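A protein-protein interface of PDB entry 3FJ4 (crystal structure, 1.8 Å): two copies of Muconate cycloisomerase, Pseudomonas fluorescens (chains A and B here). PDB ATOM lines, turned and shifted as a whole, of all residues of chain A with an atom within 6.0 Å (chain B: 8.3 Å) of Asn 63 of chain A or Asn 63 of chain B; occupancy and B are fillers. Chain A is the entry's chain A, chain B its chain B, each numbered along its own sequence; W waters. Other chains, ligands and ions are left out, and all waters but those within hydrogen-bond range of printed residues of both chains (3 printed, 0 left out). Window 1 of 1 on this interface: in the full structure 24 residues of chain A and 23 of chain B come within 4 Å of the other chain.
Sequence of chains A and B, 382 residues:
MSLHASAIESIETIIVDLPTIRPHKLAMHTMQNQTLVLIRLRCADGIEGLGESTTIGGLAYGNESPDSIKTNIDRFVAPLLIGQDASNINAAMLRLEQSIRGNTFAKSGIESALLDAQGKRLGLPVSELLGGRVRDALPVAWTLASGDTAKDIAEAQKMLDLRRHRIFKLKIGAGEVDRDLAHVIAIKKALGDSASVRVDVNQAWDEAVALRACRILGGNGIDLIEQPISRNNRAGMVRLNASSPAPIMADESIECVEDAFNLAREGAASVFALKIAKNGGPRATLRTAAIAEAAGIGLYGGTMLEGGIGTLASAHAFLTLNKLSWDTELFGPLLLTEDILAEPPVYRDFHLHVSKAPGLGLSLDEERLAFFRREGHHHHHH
The backbone carbonyl oxygen of Leu 59 of chain A lies within hydrogen-bond range of the backbone NH of Arg 101 of chain B (2.9 Å).
O of Asn 63 of chain A sits at hydrogen-bond distance from ND2 of Asn 103 of chain B.
The backbone carbonyl oxygen of Leu 59 of chain B lies within hydrogen-bond range of the backbone NH of Arg 101 of chain A.
The side-chain amide nitrogen (ND2) of Asn 72 of chain B is in hydrogen-bond range of the side-chain hydroxyl (OG) of Ser 65 of chain A (2.8 Å).
O of Asn 63 of chain B is in hydrogen-bond range of ND2 of Asn 103 of chain A, at 3.2 Å.
OG of Ser 65 of chain B lies within hydrogen-bond range of ND2 of Asn 72 of chain A, 2.8 Å away.
Water W1 lies within hydrogen-bond range of the backbone carbonyl oxygen of Asn 63 of chain B (2.8 Å) and the side-chain amide oxygen of Asn 103 of chain A (3.5 Å).
Water W3 lies within hydrogen-bond range of O of Asn 63 of chain A and OD1 of Asn 103 of chain B.
Water W2 lies within hydrogen-bond range of ND2 of Asn 63 of chain B (3.2 Å) and ND2 of Asn 63 of chain A (3.5 Å).
The side-chain amide oxygen (OD1) of Asn 72 of chain B sits close to the side-chain amide oxygen (OD1) of Asn 103 of chain B.
N of Ser 65 of chain A sits at hydrogen-bond distance from OG of Ser 68 of chain A.
The backbone NH of Ser 65 of chain B sits at hydrogen-bond distance from the side-chain hydroxyl of Ser 68 of chain B (2.9 Å).
The backbone carbonyl oxygen (O) of Arg 101 of chain A is in hydrogen-bond range of the side-chain amide nitrogen (ND2) of Asn 103 of chain A, 2.8 Å away.
OD1 of Asn 103 of chain A lies close to OD1 of Asn 72 of chain A, at 2.8 Å.
Tyr 61 of chain A touches Arg 101 of chain B, and with the chains exchanged Arg 101 of chain A touches Tyr 61 of chain B.
Asn 63 of chain B touches its own counterpart, Asn 63 of chain A.
Ser 65 of chain A touches Asn 72 of chain B, and with the chains exchanged Asn 72 of chain A touches Ser 65 of chain B.
Ser 68 of chain A touches Asn 72 of chain B, and with the chains exchanged Asn 72 of chain A touches Ser 68 of chain B.
Among the printed residues, merely in contact across the chains: Gly 58 of chain A with Phe 76 of chain B (3.7 Å), Leu 59 of chain A with Asn 72 of chain B (3.7 Å), Leu 59 of chain A with Phe 76 of chain B (3.7 Å), Leu 59 of chain A with Ile 100 of chain B (3.6 Å), Leu 59 of chain A with Asn 103 of chain B (3.9 Å), Tyr 61 of chain A with Arg 101 of chain B (3.6 Å), Gly 62 of chain A with Arg 101 of chain B (3.9 Å), Asn 63 of chain A with Asn 63 of chain B (3.99 Å), Asn 63 of chain A with Asn 72 of chain B (3.8 Å), Asn 63 of chain A with Arg 101 of chain B (3.4 Å), Ser 65 of chain A with Phe 76 of chain B (3.3 Å), Ser 68 of chain A with Asn 72 of chain B (3.4 Å), Asn 72 of chain A with Leu 59 of chain B (3.8 Å), Asn 72 of chain A with Asn 63 of chain B (3.7 Å), Asn 72 of chain A with Ser 68 of chain B (3.4 Å), Arg 101 of chain A with Ala 60 of chain B (3.4 Å), Arg 101 of chain A with Tyr 61 of chain B (3.3 Å), Arg 101 of chain A with Gly 62 of chain B (3.9 Å), Arg 101 of chain A with Asn 63 of chain B (3.5 Å) and Asn 103 of chain A with Leu 59 of chain B (3.9 Å).
Of the printed residues of chain B, Asn 63 of chain A touches Asn 63, Asn 72, Arg 101 and Asn 103.
Of the printed residues of chain A, Asn 72 of chain B touches Leu 59 (3.7 Å), Asn 63 (3.8 Å), Ser 65 (2.8 Å) and Ser 68 (3.4 Å).
Of the printed residues of chain A, Arg 101 of chain B touches Leu 59, Tyr 61, Gly 62 and Asn 63.
The nearest printed residue of chain A that does not touch Asn 63 of chain B is Gly 102 of chain A (4.3 Å).
The nearest printed residue of chain A that does not touch Leu 59 of chain B is Gly 102 of chain A (6.0 Å).
Among the printed residues, 26 pairs touch across the chains.
Among the printed residues, no Asp or Glu carboxylate lies within 4 Å of a Lys or Arg side-chain nitrogen of the other chain.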
ATOM      1  N   GLY A  58      -1.963  -1.673 -28.316  1.00  0.00           N
ATOM      2  CA  GLY A  58      -2.967  -1.585 -27.267  1.00  0.00           C
ATOM      3  C   GLY A  58      -2.958  -0.251 -26.546  1.00  0.00           C
ATOM      4  O   GLY A  58      -3.520   0.728 -27.036  1.00  0.00           O
ATOM      5  N   LEU A  59      -2.325  -0.215 -25.376  1.00  0.00           N
ATOM      6  CA  LEU A  59      -2.220   1.015 -24.596  1.00  0.00           C
ATOM      7  C   LEU A  59      -0.756   1.381 -24.388  1.00  0.00           C
ATOM      8  O   LEU A  59      -0.439   2.293 -23.624  1.00  0.00           O
ATOM      9  CB  LEU A  59      -2.894   0.856 -23.229  1.00  0.00           C
ATOM     10  CG  LEU A  59      -4.421   0.734 -23.230  1.00  0.00           C
ATOM     11  CD1 LEU A  59      -4.924   0.505 -21.813  1.00  0.00           C
ATOM     12  CD2 LEU A  59      -5.028   1.997 -23.816  1.00  0.00           C
ATOM     13  N   TYR A  61       1.210   2.714 -26.541  1.00  0.00           N
ATOM     14  CA  TYR A  61       1.568   3.949 -27.224  1.00  0.00           C
ATOM     15  C   TYR A  61       0.748   5.160 -26.767  1.00  0.00           C
ATOM     16  O   TYR A  61       1.306   6.228 -26.506  1.00  0.00           O
ATOM     17  CB  TYR A  61       1.421   3.773 -28.735  1.00  0.00           C
ATOM     18  CG  TYR A  61       2.004   4.918 -29.526  1.00  0.00           C
ATOM     19  CD1 TYR A  61       3.240   4.796 -30.159  1.00  0.00           C
ATOM     20  CD2 TYR A  61       1.328   6.136 -29.625  1.00  0.00           C
ATOM     21  CE1 TYR A  61       3.786   5.857 -30.878  1.00  0.00           C
ATOM     22  CE2 TYR A  61       1.868   7.204 -30.336  1.00  0.00           C
ATOM     23  CZ  TYR A  61       3.092   7.057 -30.961  1.00  0.00           C
ATOM     24  OH  TYR A  61       3.611   8.101 -31.685  1.00  0.00           O
ATOM     25  N   GLY A  62      -0.568   4.994 -26.678  1.00  0.00           N
ATOM     26  CA  GLY A  62      -1.434   6.085 -26.260  1.00  0.00           C
ATOM     27  C   GLY A  62      -2.484   5.603 -25.274  1.00  0.00           C
ATOM     28  O   GLY A  62      -2.586   4.402 -25.019  1.00  0.00           O
ATOM     29  N   ASN A  63      -3.282   6.519 -24.733  1.00  0.00           N
ATOM     30  CA  ASN A  63      -4.297   6.137 -23.752  1.00  0.00           C
ATOM     31  C   ASN A  63      -5.568   5.512 -24.330  1.00  0.00           C
ATOM     32  O   ASN A  63      -6.429   5.048 -23.581  1.00  0.00           O
ATOM     33  CB  ASN A  63      -4.660   7.334 -22.864  1.00  0.00           C
ATOM     34  CG  ASN A  63      -5.131   8.531 -23.660  1.00  0.00           C
ATOM     35  OD1 ASN A  63      -5.975   8.412 -24.541  1.00  0.00           O
ATOM     36  ND2 ASN A  63      -4.594   9.699 -23.341  1.00  0.00           N
ATOM     37  N   GLU A  64      -5.694   5.506 -25.653  1.00  0.00           N
ATOM     38  CA  GLU A  64      -6.860   4.903 -26.300  1.00  0.00           C
ATOM     39  C   GLU A  64      -6.474   3.574 -26.948  1.00  0.00           C
ATOM     40  O   GLU A  64      -5.501   3.506 -27.702  1.00  0.00           O
ATOM     41  CB  GLU A  64      -7.425   5.817 -27.396  1.00  0.00           C
ATOM     42  CG  GLU A  64      -8.009   7.140 -26.916  1.00  0.00           C
ATOM     43  CD  GLU A  64      -8.376   8.061 -28.071  1.00  0.00           C
ATOM     44  OE1 GLU A  64      -9.440   7.854 -28.705  1.00  0.00           O
ATOM     45  OE2 GLU A  64      -7.590   8.989 -28.358  1.00  0.00           O
ATOM     46  N   SER A  65      -7.232   2.520 -26.654  1.00  0.00           N
ATOM     47  CA  SER A  65      -6.975   1.213 -27.255  1.00  0.00           C
ATOM     48  C   SER A  65      -8.080   0.975 -28.276  1.00  0.00           C
ATOM     49  O   SER A  65      -9.105   1.654 -28.251  1.00  0.00           O
ATOM     50  CB  SER A  65      -7.029   0.100 -26.203  1.00  0.00           C
ATOM     51  OG  SER A  65      -8.315   0.024 -25.609  1.00  0.00           O
ATOM     52  N   SER A  68     -11.163   0.447 -26.205  1.00  0.00           N
ATOM     53  CA  SER A  68     -11.798   1.598 -25.561  1.00  0.00           C
ATOM     54  C   SER A  68     -12.353   2.599 -26.573  1.00  0.00           C
ATOM     55  O   SER A  68     -13.302   3.329 -26.280  1.00  0.00           O
ATOM     56  CB  SER A  68     -10.830   2.289 -24.583  1.00  0.00           C
ATOM     57  OG  SER A  68      -9.757   2.932 -25.244  1.00  0.00           O
ATOM     58  N   ASN A  72     -16.120   3.969 -26.219  1.00  0.00           N
ATOM     59  CA  ASN A  72     -16.470   5.383 -26.136  1.00  0.00           C
ATOM     60  C   ASN A  72     -17.257   5.897 -27.342  1.00  0.00           C
ATOM     61  O   ASN A  72     -18.122   6.762 -27.195  1.00  0.00           O
ATOM     62  CB  ASN A  72     -15.208   6.228 -25.905  1.00  0.00           C
ATOM     63  CG  ASN A  72     -14.770   6.238 -24.450  1.00  0.00           C
ATOM     64  OD1 ASN A  72     -13.666   6.685 -24.126  1.00  0.00           O
ATOM     65  ND2 ASN A  72     -15.638   5.762 -23.560  1.00  0.00           N
ATOM     66  N   ARG A 101     -14.181  15.095 -23.949  1.00  0.00           N
ATOM     67  CA  ARG A 101     -12.808  15.537 -23.755  1.00  0.00           C
ATOM     68  C   ARG A 101     -11.848  14.475 -24.284  1.00  0.00           C
ATOM     69  O   ARG A 101     -12.074  13.282 -24.089  1.00  0.00           O
ATOM     70  CB  ARG A 101     -12.539  15.768 -22.269  1.00  0.00           C
ATOM     71  CG  ARG A 101     -13.425  16.814 -21.615  1.00  0.00           C
ATOM     72  CD  ARG A 101     -13.055  18.244 -22.017  1.00  0.00           C
ATOM     73  NE  ARG A 101     -13.523  18.620 -23.354  1.00  0.00           N
ATOM     74  CZ  ARG A 101     -12.773  18.607 -24.453  1.00  0.00           C
ATOM     75  NH1 ARG A 101     -11.500  18.233 -24.396  1.00  0.00           N
ATOM     76  NH2 ARG A 101     -13.295  18.983 -25.614  1.00  0.00           N
ATOM     77  N   GLY A 102     -10.783  14.914 -24.950  1.00  0.00           N
ATOM     78  CA  GLY A 102      -9.806  13.977 -25.482  1.00  0.00           C
ATOM     79  C   GLY A 102     -10.378  13.033 -26.528  1.00  0.00           C
ATOM     80  O   GLY A 102     -11.121  13.457 -27.411  1.00  0.00           O
ATOM     81  N   ASN A 103     -10.009  11.758 -26.444  1.00  0.00           N
ATOM     82  CA  ASN A 103     -10.500  10.761 -27.392  1.00  0.00           C
ATOM     83  C   ASN A 103     -10.273  11.215 -28.828  1.00  0.00           C
ATOM     84  O   ASN A 103     -11.166  11.095 -29.667  1.00  0.00           O
ATOM     85  CB  ASN A 103     -11.999  10.528 -27.163  1.00  0.00           C
ATOM     86  CG  ASN A 103     -12.286   9.795 -25.870  1.00  0.00           C
ATOM     87  OD1 ASN A 103     -12.431   8.574 -25.853  1.00  0.00           O
ATOM     88  ND2 ASN A 103     -12.358  10.538 -24.773  1.00  0.00           N
ATOM     89  N   GLU A 255      -0.462  16.164 -28.580  1.00  0.00           N
ATOM     90  CA  GLU A 255      -1.610  15.301 -28.309  1.00  0.00           C
ATOM     91  C   GLU A 255      -2.916  16.068 -28.527  1.00  0.00           C
ATOM     92  O   GLU A 255      -4.001  15.595 -28.188  1.00  0.00           O
ATOM     93  CB  GLU A 255      -1.540  14.732 -26.883  1.00  0.00           C
ATOM     94  CG  GLU A 255      -0.315  13.849 -26.650  1.00  0.00           C
ATOM     95  CD  GLU A 255      -0.327  13.150 -25.298  1.00  0.00           C
ATOM     96  OE1 GLU A 255      -0.900  13.703 -24.336  1.00  0.00           O
ATOM     97  OE2 GLU A 255       0.259  12.052 -25.194  1.00  0.00           O
ATOM     98  N   THR B  55     -15.513   9.200 -12.303  1.00  0.00           N
ATOM     99  CA  THR B  55     -15.302  10.476 -12.964  1.00  0.00           C
ATOM    100  C   THR B  55     -16.610  11.261 -12.943  1.00  0.00           C
ATOM    101  O   THR B  55     -17.502  10.962 -12.144  1.00  0.00           O
ATOM    102  CB  THR B  55     -14.799  10.309 -14.419  1.00  0.00           C
ATOM    103  OG1 THR B  55     -14.502  11.601 -14.968  1.00  0.00           O
ATOM    104  CG2 THR B  55     -15.846   9.620 -15.287  1.00  0.00           C
ATOM    105  N   ILE B  56     -16.724  12.260 -13.810  1.00  0.00           N
ATOM    106  CA  ILE B  56     -17.924  13.089 -13.853  1.00  0.00           C
ATOM    107  C   ILE B  56     -18.475  13.283 -15.260  1.00  0.00           C
ATOM    108  O   ILE B  56     -17.741  13.640 -16.177  1.00  0.00           O
ATOM    109  CB  ILE B  56     -17.640  14.487 -13.245  1.00  0.00           C
ATOM    110  CG1 ILE B  56     -17.323  14.347 -11.754  1.00  0.00           C
ATOM    111  CG2 ILE B  56     -18.828  15.410 -13.471  1.00  0.00           C
ATOM    112  CD1 ILE B  56     -16.820  15.610 -11.112  1.00  0.00           C
ATOM    113  N   GLY B  58     -19.649  11.174 -17.760  1.00  0.00           N
ATOM    114  CA  GLY B  58     -19.204  10.380 -18.892  1.00  0.00           C
ATOM    115  C   GLY B  58     -17.829  10.783 -19.391  1.00  0.00           C
ATOM    116  O   GLY B  58     -16.819  10.377 -18.821  1.00  0.00           O
ATOM    117  N   LEU B  59     -17.800  11.568 -20.464  1.00  0.00           N
ATOM    118  CA  LEU B  59     -16.554  12.059 -21.049  1.00  0.00           C
ATOM    119  C   LEU B  59     -16.554  13.586 -21.047  1.00  0.00           C
ATOM    120  O   LEU B  59     -15.704  14.214 -21.677  1.00  0.00           O
ATOM    121  CB  LEU B  59     -16.403  11.557 -22.494  1.00  0.00           C
ATOM    122  CG  LEU B  59     -16.217  10.050 -22.694  1.00  0.00           C
ATOM    123  CD1 LEU B  59     -16.149   9.721 -24.185  1.00  0.00           C
ATOM    124  CD2 LEU B  59     -14.942   9.600 -21.989  1.00  0.00           C
ATOM    125  N   ALA B  60     -17.510  14.177 -20.337  1.00  0.00           N
ATOM    126  CA  ALA B  60     -17.632  15.632 -20.275  1.00  0.00           C
ATOM    127  C   ALA B  60     -16.510  16.282 -19.483  1.00  0.00           C
ATOM    128  O   ALA B  60     -16.172  17.448 -19.697  1.00  0.00           O
ATOM    129  CB  ALA B  60     -18.977  16.014 -19.664  1.00  0.00           C
ATOM    130  N   TYR B  61     -15.933  15.522 -18.567  1.00  0.00           N
ATOM    131  CA  TYR B  61     -14.874  16.042 -17.724  1.00  0.00           C
ATOM    132  C   TYR B  61     -13.492  15.589 -18.184  1.00  0.00           C
ATOM    133  O   TYR B  61     -12.611  16.419 -18.413  1.00  0.00           O
ATOM    134  CB  TYR B  61     -15.107  15.606 -16.279  1.00  0.00           C
ATOM    135  CG  TYR B  61     -14.237  16.336 -15.287  1.00  0.00           C
ATOM    136  CD1 TYR B  61     -14.731  17.420 -14.563  1.00  0.00           C
ATOM    137  CD2 TYR B  61     -12.910  15.958 -15.088  1.00  0.00           C
ATOM    138  CE1 TYR B  61     -13.923  18.110 -13.659  1.00  0.00           C
ATOM    139  CE2 TYR B  61     -12.092  16.643 -14.191  1.00  0.00           C
ATOM    140  CZ  TYR B  61     -12.606  17.714 -13.482  1.00  0.00           C
ATOM    141  OH  TYR B  61     -11.799  18.385 -12.594  1.00  0.00           O
ATOM    142  N   GLY B  62     -13.313  14.276 -18.324  1.00  0.00           N
ATOM    143  CA  GLY B  62     -12.032  13.735 -18.746  1.00  0.00           C
ATOM    144  C   GLY B  62     -12.155  12.743 -19.889  1.00  0.00           C
ATOM    145  O   GLY B  62     -13.259  12.459 -20.358  1.00  0.00           O
ATOM    146  N   ASN B  63     -11.027  12.197 -20.334  1.00  0.00           N
ATOM    147  CA  ASN B  63     -11.045  11.257 -21.453  1.00  0.00           C
ATOM    148  C   ASN B  63     -11.446   9.824 -21.109  1.00  0.00           C
ATOM    149  O   ASN B  63     -11.692   9.021 -22.007  1.00  0.00           O
ATOM    150  CB  ASN B  63      -9.688  11.251 -22.165  1.00  0.00           C
ATOM    151  CG  ASN B  63      -8.543  10.920 -21.234  1.00  0.00           C
ATOM    152  OD1 ASN B  63      -8.638  10.005 -20.422  1.00  0.00           O
ATOM    153  ND2 ASN B  63      -7.446  11.659 -21.355  1.00  0.00           N
ATOM    154  N   GLU B  64     -11.499   9.492 -19.822  1.00  0.00           N
ATOM    155  CA  GLU B  64     -11.900   8.147 -19.412  1.00  0.00           C
ATOM    156  C   GLU B  64     -13.336   8.176 -18.911  1.00  0.00           C
ATOM    157  O   GLU B  64     -13.703   9.039 -18.121  1.00  0.00           O
ATOM    158  CB  GLU B  64     -11.013   7.611 -18.282  1.00  0.00           C
ATOM    159  CG  GLU B  64      -9.555   7.390 -18.641  1.00  0.00           C
ATOM    160  CD  GLU B  64      -8.708   7.072 -17.417  1.00  0.00           C
ATOM    161  OE1 GLU B  64      -8.764   5.921 -16.918  1.00  0.00           O
ATOM    162  OE2 GLU B  64      -7.995   7.984 -16.943  1.00  0.00           O
ATOM    163  N   SER B  65     -14.147   7.236 -19.381  1.00  0.00           N
ATOM    164  CA  SER B  65     -15.532   7.147 -18.947  1.00  0.00           C
ATOM    165  C   SER B  65     -15.627   5.898 -18.080  1.00  0.00           C
ATOM    166  O   SER B  65     -14.739   5.048 -18.106  1.00  0.00           O
ATOM    167  CB  SER B  65     -16.459   7.001 -20.155  1.00  0.00           C
ATOM    168  OG  SER B  65     -16.236   5.756 -20.794  1.00  0.00           O
ATOM    169  N   PRO B  66     -16.698   5.770 -17.285  1.00  0.00           N
ATOM    170  CA  PRO B  66     -16.783   4.563 -16.460  1.00  0.00           C
ATOM    171  C   PRO B  66     -16.689   3.335 -17.369  1.00  0.00           C
ATOM    172  O   PRO B  66     -16.085   2.320 -17.023  1.00  0.00           O
ATOM    173  CB  PRO B  66     -18.160   4.691 -15.813  1.00  0.00           C
ATOM    174  CG  PRO B  66     -18.340   6.190 -15.694  1.00  0.00           C
ATOM    175  CD  PRO B  66     -17.832   6.677 -17.035  1.00  0.00           C
ATOM    176  N   SER B  68     -15.175   3.041 -20.515  1.00  0.00           N
ATOM    177  CA  SER B  68     -13.858   2.770 -21.087  1.00  0.00           C
ATOM    178  C   SER B  68     -12.883   2.315 -20.005  1.00  0.00           C
ATOM    179  O   SER B  68     -11.936   1.577 -20.282  1.00  0.00           O
ATOM    180  CB  SER B  68     -13.310   4.005 -21.833  1.00  0.00           C
ATOM    181  OG  SER B  68     -13.099   5.112 -20.976  1.00  0.00           O
ATOM    182  N   ILE B  69     -13.119   2.747 -18.769  1.00  0.00           N
ATOM    183  CA  ILE B  69     -12.267   2.341 -17.657  1.00  0.00           C
ATOM    184  C   ILE B  69     -12.432   0.829 -17.488  1.00  0.00           C
ATOM    185  O   ILE B  69     -11.451   0.091 -17.354  1.00  0.00           O
ATOM    186  CB  ILE B  69     -12.674   3.062 -16.341  1.00  0.00           C
ATOM    187  CG1 ILE B  69     -12.305   4.545 -16.424  1.00  0.00           C
ATOM    188  CG2 ILE B  69     -11.975   2.416 -15.150  1.00  0.00           C
ATOM    189  CD1 ILE B  69     -12.929   5.405 -15.321  1.00  0.00           C
ATOM    190  N   ASN B  72     -10.656  -0.979 -20.551  1.00  0.00           N
ATOM    191  CA  ASN B  72      -9.202  -1.019 -20.477  1.00  0.00           C
ATOM    192  C   ASN B  72      -8.659  -1.823 -19.304  1.00  0.00           C
ATOM    193  O   ASN B  72      -7.591  -2.418 -19.411  1.00  0.00           O
ATOM    194  CB  ASN B  72      -8.630   0.409 -20.481  1.00  0.00           C
ATOM    195  CG  ASN B  72      -8.585   1.007 -21.878  1.00  0.00           C
ATOM    196  OD1 ASN B  72      -8.404   2.217 -22.054  1.00  0.00           O
ATOM    197  ND2 ASN B  72      -8.737   0.159 -22.882  1.00  0.00           N
ATOM    198  N   PHE B  76      -6.658  -4.859 -20.659  1.00  0.00           N
ATOM    199  CA  PHE B  76      -5.220  -4.622 -20.548  1.00  0.00           C
ATOM    200  C   PHE B  76      -4.571  -4.701 -19.171  1.00  0.00           C
ATOM    201  O   PHE B  76      -3.463  -5.218 -19.042  1.00  0.00           O
ATOM    202  CB  PHE B  76      -4.889  -3.276 -21.197  1.00  0.00           C
ATOM    203  CG  PHE B  76      -5.202  -3.237 -22.658  1.00  0.00           C
ATOM    204  CD1 PHE B  76      -4.342  -3.826 -23.583  1.00  0.00           C
ATOM    205  CD2 PHE B  76      -6.389  -2.683 -23.109  1.00  0.00           C
ATOM    206  CE1 PHE B  76      -4.668  -3.866 -24.935  1.00  0.00           C
ATOM    207  CE2 PHE B  76      -6.725  -2.720 -24.458  1.00  0.00           C
ATOM    208  CZ  PHE B  76      -5.863  -3.314 -25.373  1.00  0.00           C
ATOM    209  N   ILE B 100       1.213   0.644 -20.051  1.00  0.00           N
ATOM    210  CA  ILE B 100      -0.021   1.407 -20.189  1.00  0.00           C
ATOM    211  C   ILE B 100       0.155   2.908 -20.042  1.00  0.00           C
ATOM    212  O   ILE B 100       0.536   3.399 -18.980  1.00  0.00           O
ATOM    213  CB  ILE B 100      -1.071   0.928 -19.159  1.00  0.00           C
ATOM    214  CG1 ILE B 100      -1.367  -0.559 -19.386  1.00  0.00           C
ATOM    215  CG2 ILE B 100      -2.337   1.771 -19.274  1.00  0.00           C
ATOM    216  CD1 ILE B 100      -2.419  -1.145 -18.469  1.00  0.00           C
ATOM    217  N   ARG B 101      -0.138   3.633 -21.115  1.00  0.00           N
ATOM    218  CA  ARG B 101      -0.019   5.086 -21.114  1.00  0.00           C
ATOM    219  C   ARG B 101      -1.326   5.714 -20.641  1.00  0.00           C
ATOM    220  O   ARG B 101      -2.410   5.263 -21.016  1.00  0.00           O
ATOM    221  CB  ARG B 101       0.314   5.591 -22.525  1.00  0.00           C
ATOM    222  CG  ARG B 101       1.604   5.021 -23.127  1.00  0.00           C
ATOM    223  CD  ARG B 101       2.840   5.483 -22.367  1.00  0.00           C
ATOM    224  NE  ARG B 101       2.742   5.126 -20.956  1.00  0.00           N
ATOM    225  CZ  ARG B 101       3.615   5.482 -20.022  1.00  0.00           C
ATOM    226  NH1 ARG B 101       4.677   6.214 -20.339  1.00  0.00           N
ATOM    227  NH2 ARG B 101       3.410   5.120 -18.764  1.00  0.00           N
ATOM    228  N   GLY B 102      -1.219   6.753 -19.815  1.00  0.00           N
ATOM    229  CA  GLY B 102      -2.405   7.426 -19.316  1.00  0.00           C
ATOM    230  C   GLY B 102      -3.275   6.525 -18.455  1.00  0.00           C
ATOM    231  O   GLY B 102      -2.767   5.767 -17.631  1.00  0.00           O
ATOM    232  N   ASN B 103      -4.590   6.620 -18.635  1.00  0.00           N
ATOM    233  CA  ASN B 103      -5.519   5.795 -17.869  1.00  0.00           C
ATOM    234  C   ASN B 103      -5.286   5.923 -16.364  1.00  0.00           C
ATOM    235  O   ASN B 103      -5.297   4.928 -15.639  1.00  0.00           O
ATOM    236  CB  ASN B 103      -5.377   4.330 -18.301  1.00  0.00           C
ATOM    237  CG  ASN B 103      -5.919   4.084 -19.695  1.00  0.00           C
ATOM    238  OD1 ASN B 103      -7.073   3.694 -19.861  1.00  0.00           O
ATOM    239  ND2 ASN B 103      -5.092   4.330 -20.707  1.00  0.00           N
ATOM    240  N   THR B 104      -5.089   7.151 -15.894  1.00  0.00           N
ATOM    241  CA  THR B 104      -4.853   7.385 -14.473  1.00  0.00           C
ATOM    242  C   THR B 104      -6.052   7.025 -13.595  1.00  0.00           C
ATOM    243  O   THR B 104      -5.872   6.537 -12.476  1.00  0.00           O
ATOM    244  CB  THR B 104      -4.470   8.856 -14.191  1.00  0.00           C
ATOM    245  OG1 THR B 104      -5.511   9.720 -14.658  1.00  0.00           O
ATOM    246  CG2 THR B 104      -3.157   9.205 -14.888  1.00  0.00           C
ATOM    247  N   PHE B 105      -7.267   7.271 -14.083  1.00  0.00           N
ATOM    248  CA  PHE B 105      -8.456   6.939 -13.295  1.00  0.00           C
ATOM    249  C   PHE B 105      -8.469   5.436 -13.014  1.00  0.00           C
ATOM    250  O   PHE B 105      -8.693   5.006 -11.880  1.00  0.00           O
ATOM    251  CB  PHE B 105      -9.741   7.343 -14.033  1.00  0.00           C
ATOM    252  CG  PHE B 105     -10.051   8.818 -13.968  1.00  0.00           C
ATOM    253  CD1 PHE B 105      -9.206   9.754 -14.561  1.00  0.00           C
ATOM    254  CD2 PHE B 105     -11.195   9.272 -13.315  1.00  0.00           C
ATOM    255  CE1 PHE B 105      -9.496  11.116 -14.510  1.00  0.00           C
ATOM    256  CE2 PHE B 105     -11.495  10.633 -13.257  1.00  0.00           C
ATOM    257  CZ  PHE B 105     -10.646  11.557 -13.855  1.00  0.00           C
ATOM    258  N   LYS B 107      -5.856   3.330 -13.181  1.00  0.00           N
ATOM    259  CA  LYS B 107      -4.711   3.012 -12.333  1.00  0.00           C
ATOM    260  C   LYS B 107      -4.999   3.358 -10.878  1.00  0.00           C
ATOM    261  O   LYS B 107      -4.567   2.651  -9.969  1.00  0.00           O
ATOM    262  CB  LYS B 107      -3.461   3.771 -12.809  1.00  0.00           C
ATOM    263  CG  LYS B 107      -2.875   3.255 -14.133  1.00  0.00           C
ATOM    264  CD  LYS B 107      -1.805   4.197 -14.693  1.00  0.00           C
ATOM    265  CE  LYS B 107      -1.135   3.608 -15.938  1.00  0.00           C
ATOM    266  NZ  LYS B 107      -0.294   4.621 -16.656  1.00  0.00           N
ATOM    267  N   GLU B 255      -2.830  16.506 -14.872  1.00  0.00           N
ATOM    268  CA  GLU B 255      -3.372  15.253 -15.393  1.00  0.00           C
ATOM    269  C   GLU B 255      -2.353  14.131 -15.216  1.00  0.00           C
ATOM    270  O   GLU B 255      -2.521  13.028 -15.733  1.00  0.00           O
ATOM    271  CB  GLU B 255      -3.765  15.400 -16.868  1.00  0.00           C
ATOM    272  CG  GLU B 255      -4.818  16.474 -17.098  1.00  0.00           C
ATOM    273  CD  GLU B 255      -5.398  16.456 -18.503  1.00  0.00           C
ATOM    274  OE1 GLU B 255      -4.654  16.152 -19.459  1.00  0.00           O
ATOM    275  OE2 GLU B 255      -6.601  16.761 -18.649  1.00  0.00           O
ATOM    276  N   LYS B 278      -6.594  11.743 -10.954  1.00  0.00           N
ATOM    277  CA  LYS B 278      -5.813  12.483 -11.946  1.00  0.00           C
ATOM    278  C   LYS B 278      -4.325  12.138 -11.935  1.00  0.00           C
ATOM    279  O   LYS B 278      -3.629  12.344 -12.928  1.00  0.00           O
ATOM    280  CB  LYS B 278      -5.971  13.993 -11.726  1.00  0.00           C
ATOM    281  CG  LYS B 278      -7.407  14.511 -11.767  1.00  0.00           C
ATOM    282  CD  LYS B 278      -8.074  14.256 -13.110  1.00  0.00           C
ATOM    283  CE  LYS B 278      -7.322  14.916 -14.253  1.00  0.00           C
ATOM    284  NZ  LYS B 278      -7.287  16.406 -14.135  1.00  0.00           N
HETATM  285  O   HOH W   1     -10.093   7.402 -23.584  1.00  0.00           O
HETATM  286  O   HOH W   2      -6.496  12.452 -24.334  1.00  0.00           O
HETATM  287  O   HOH W   3      -8.450   5.979 -21.889  1.00  0.00           O
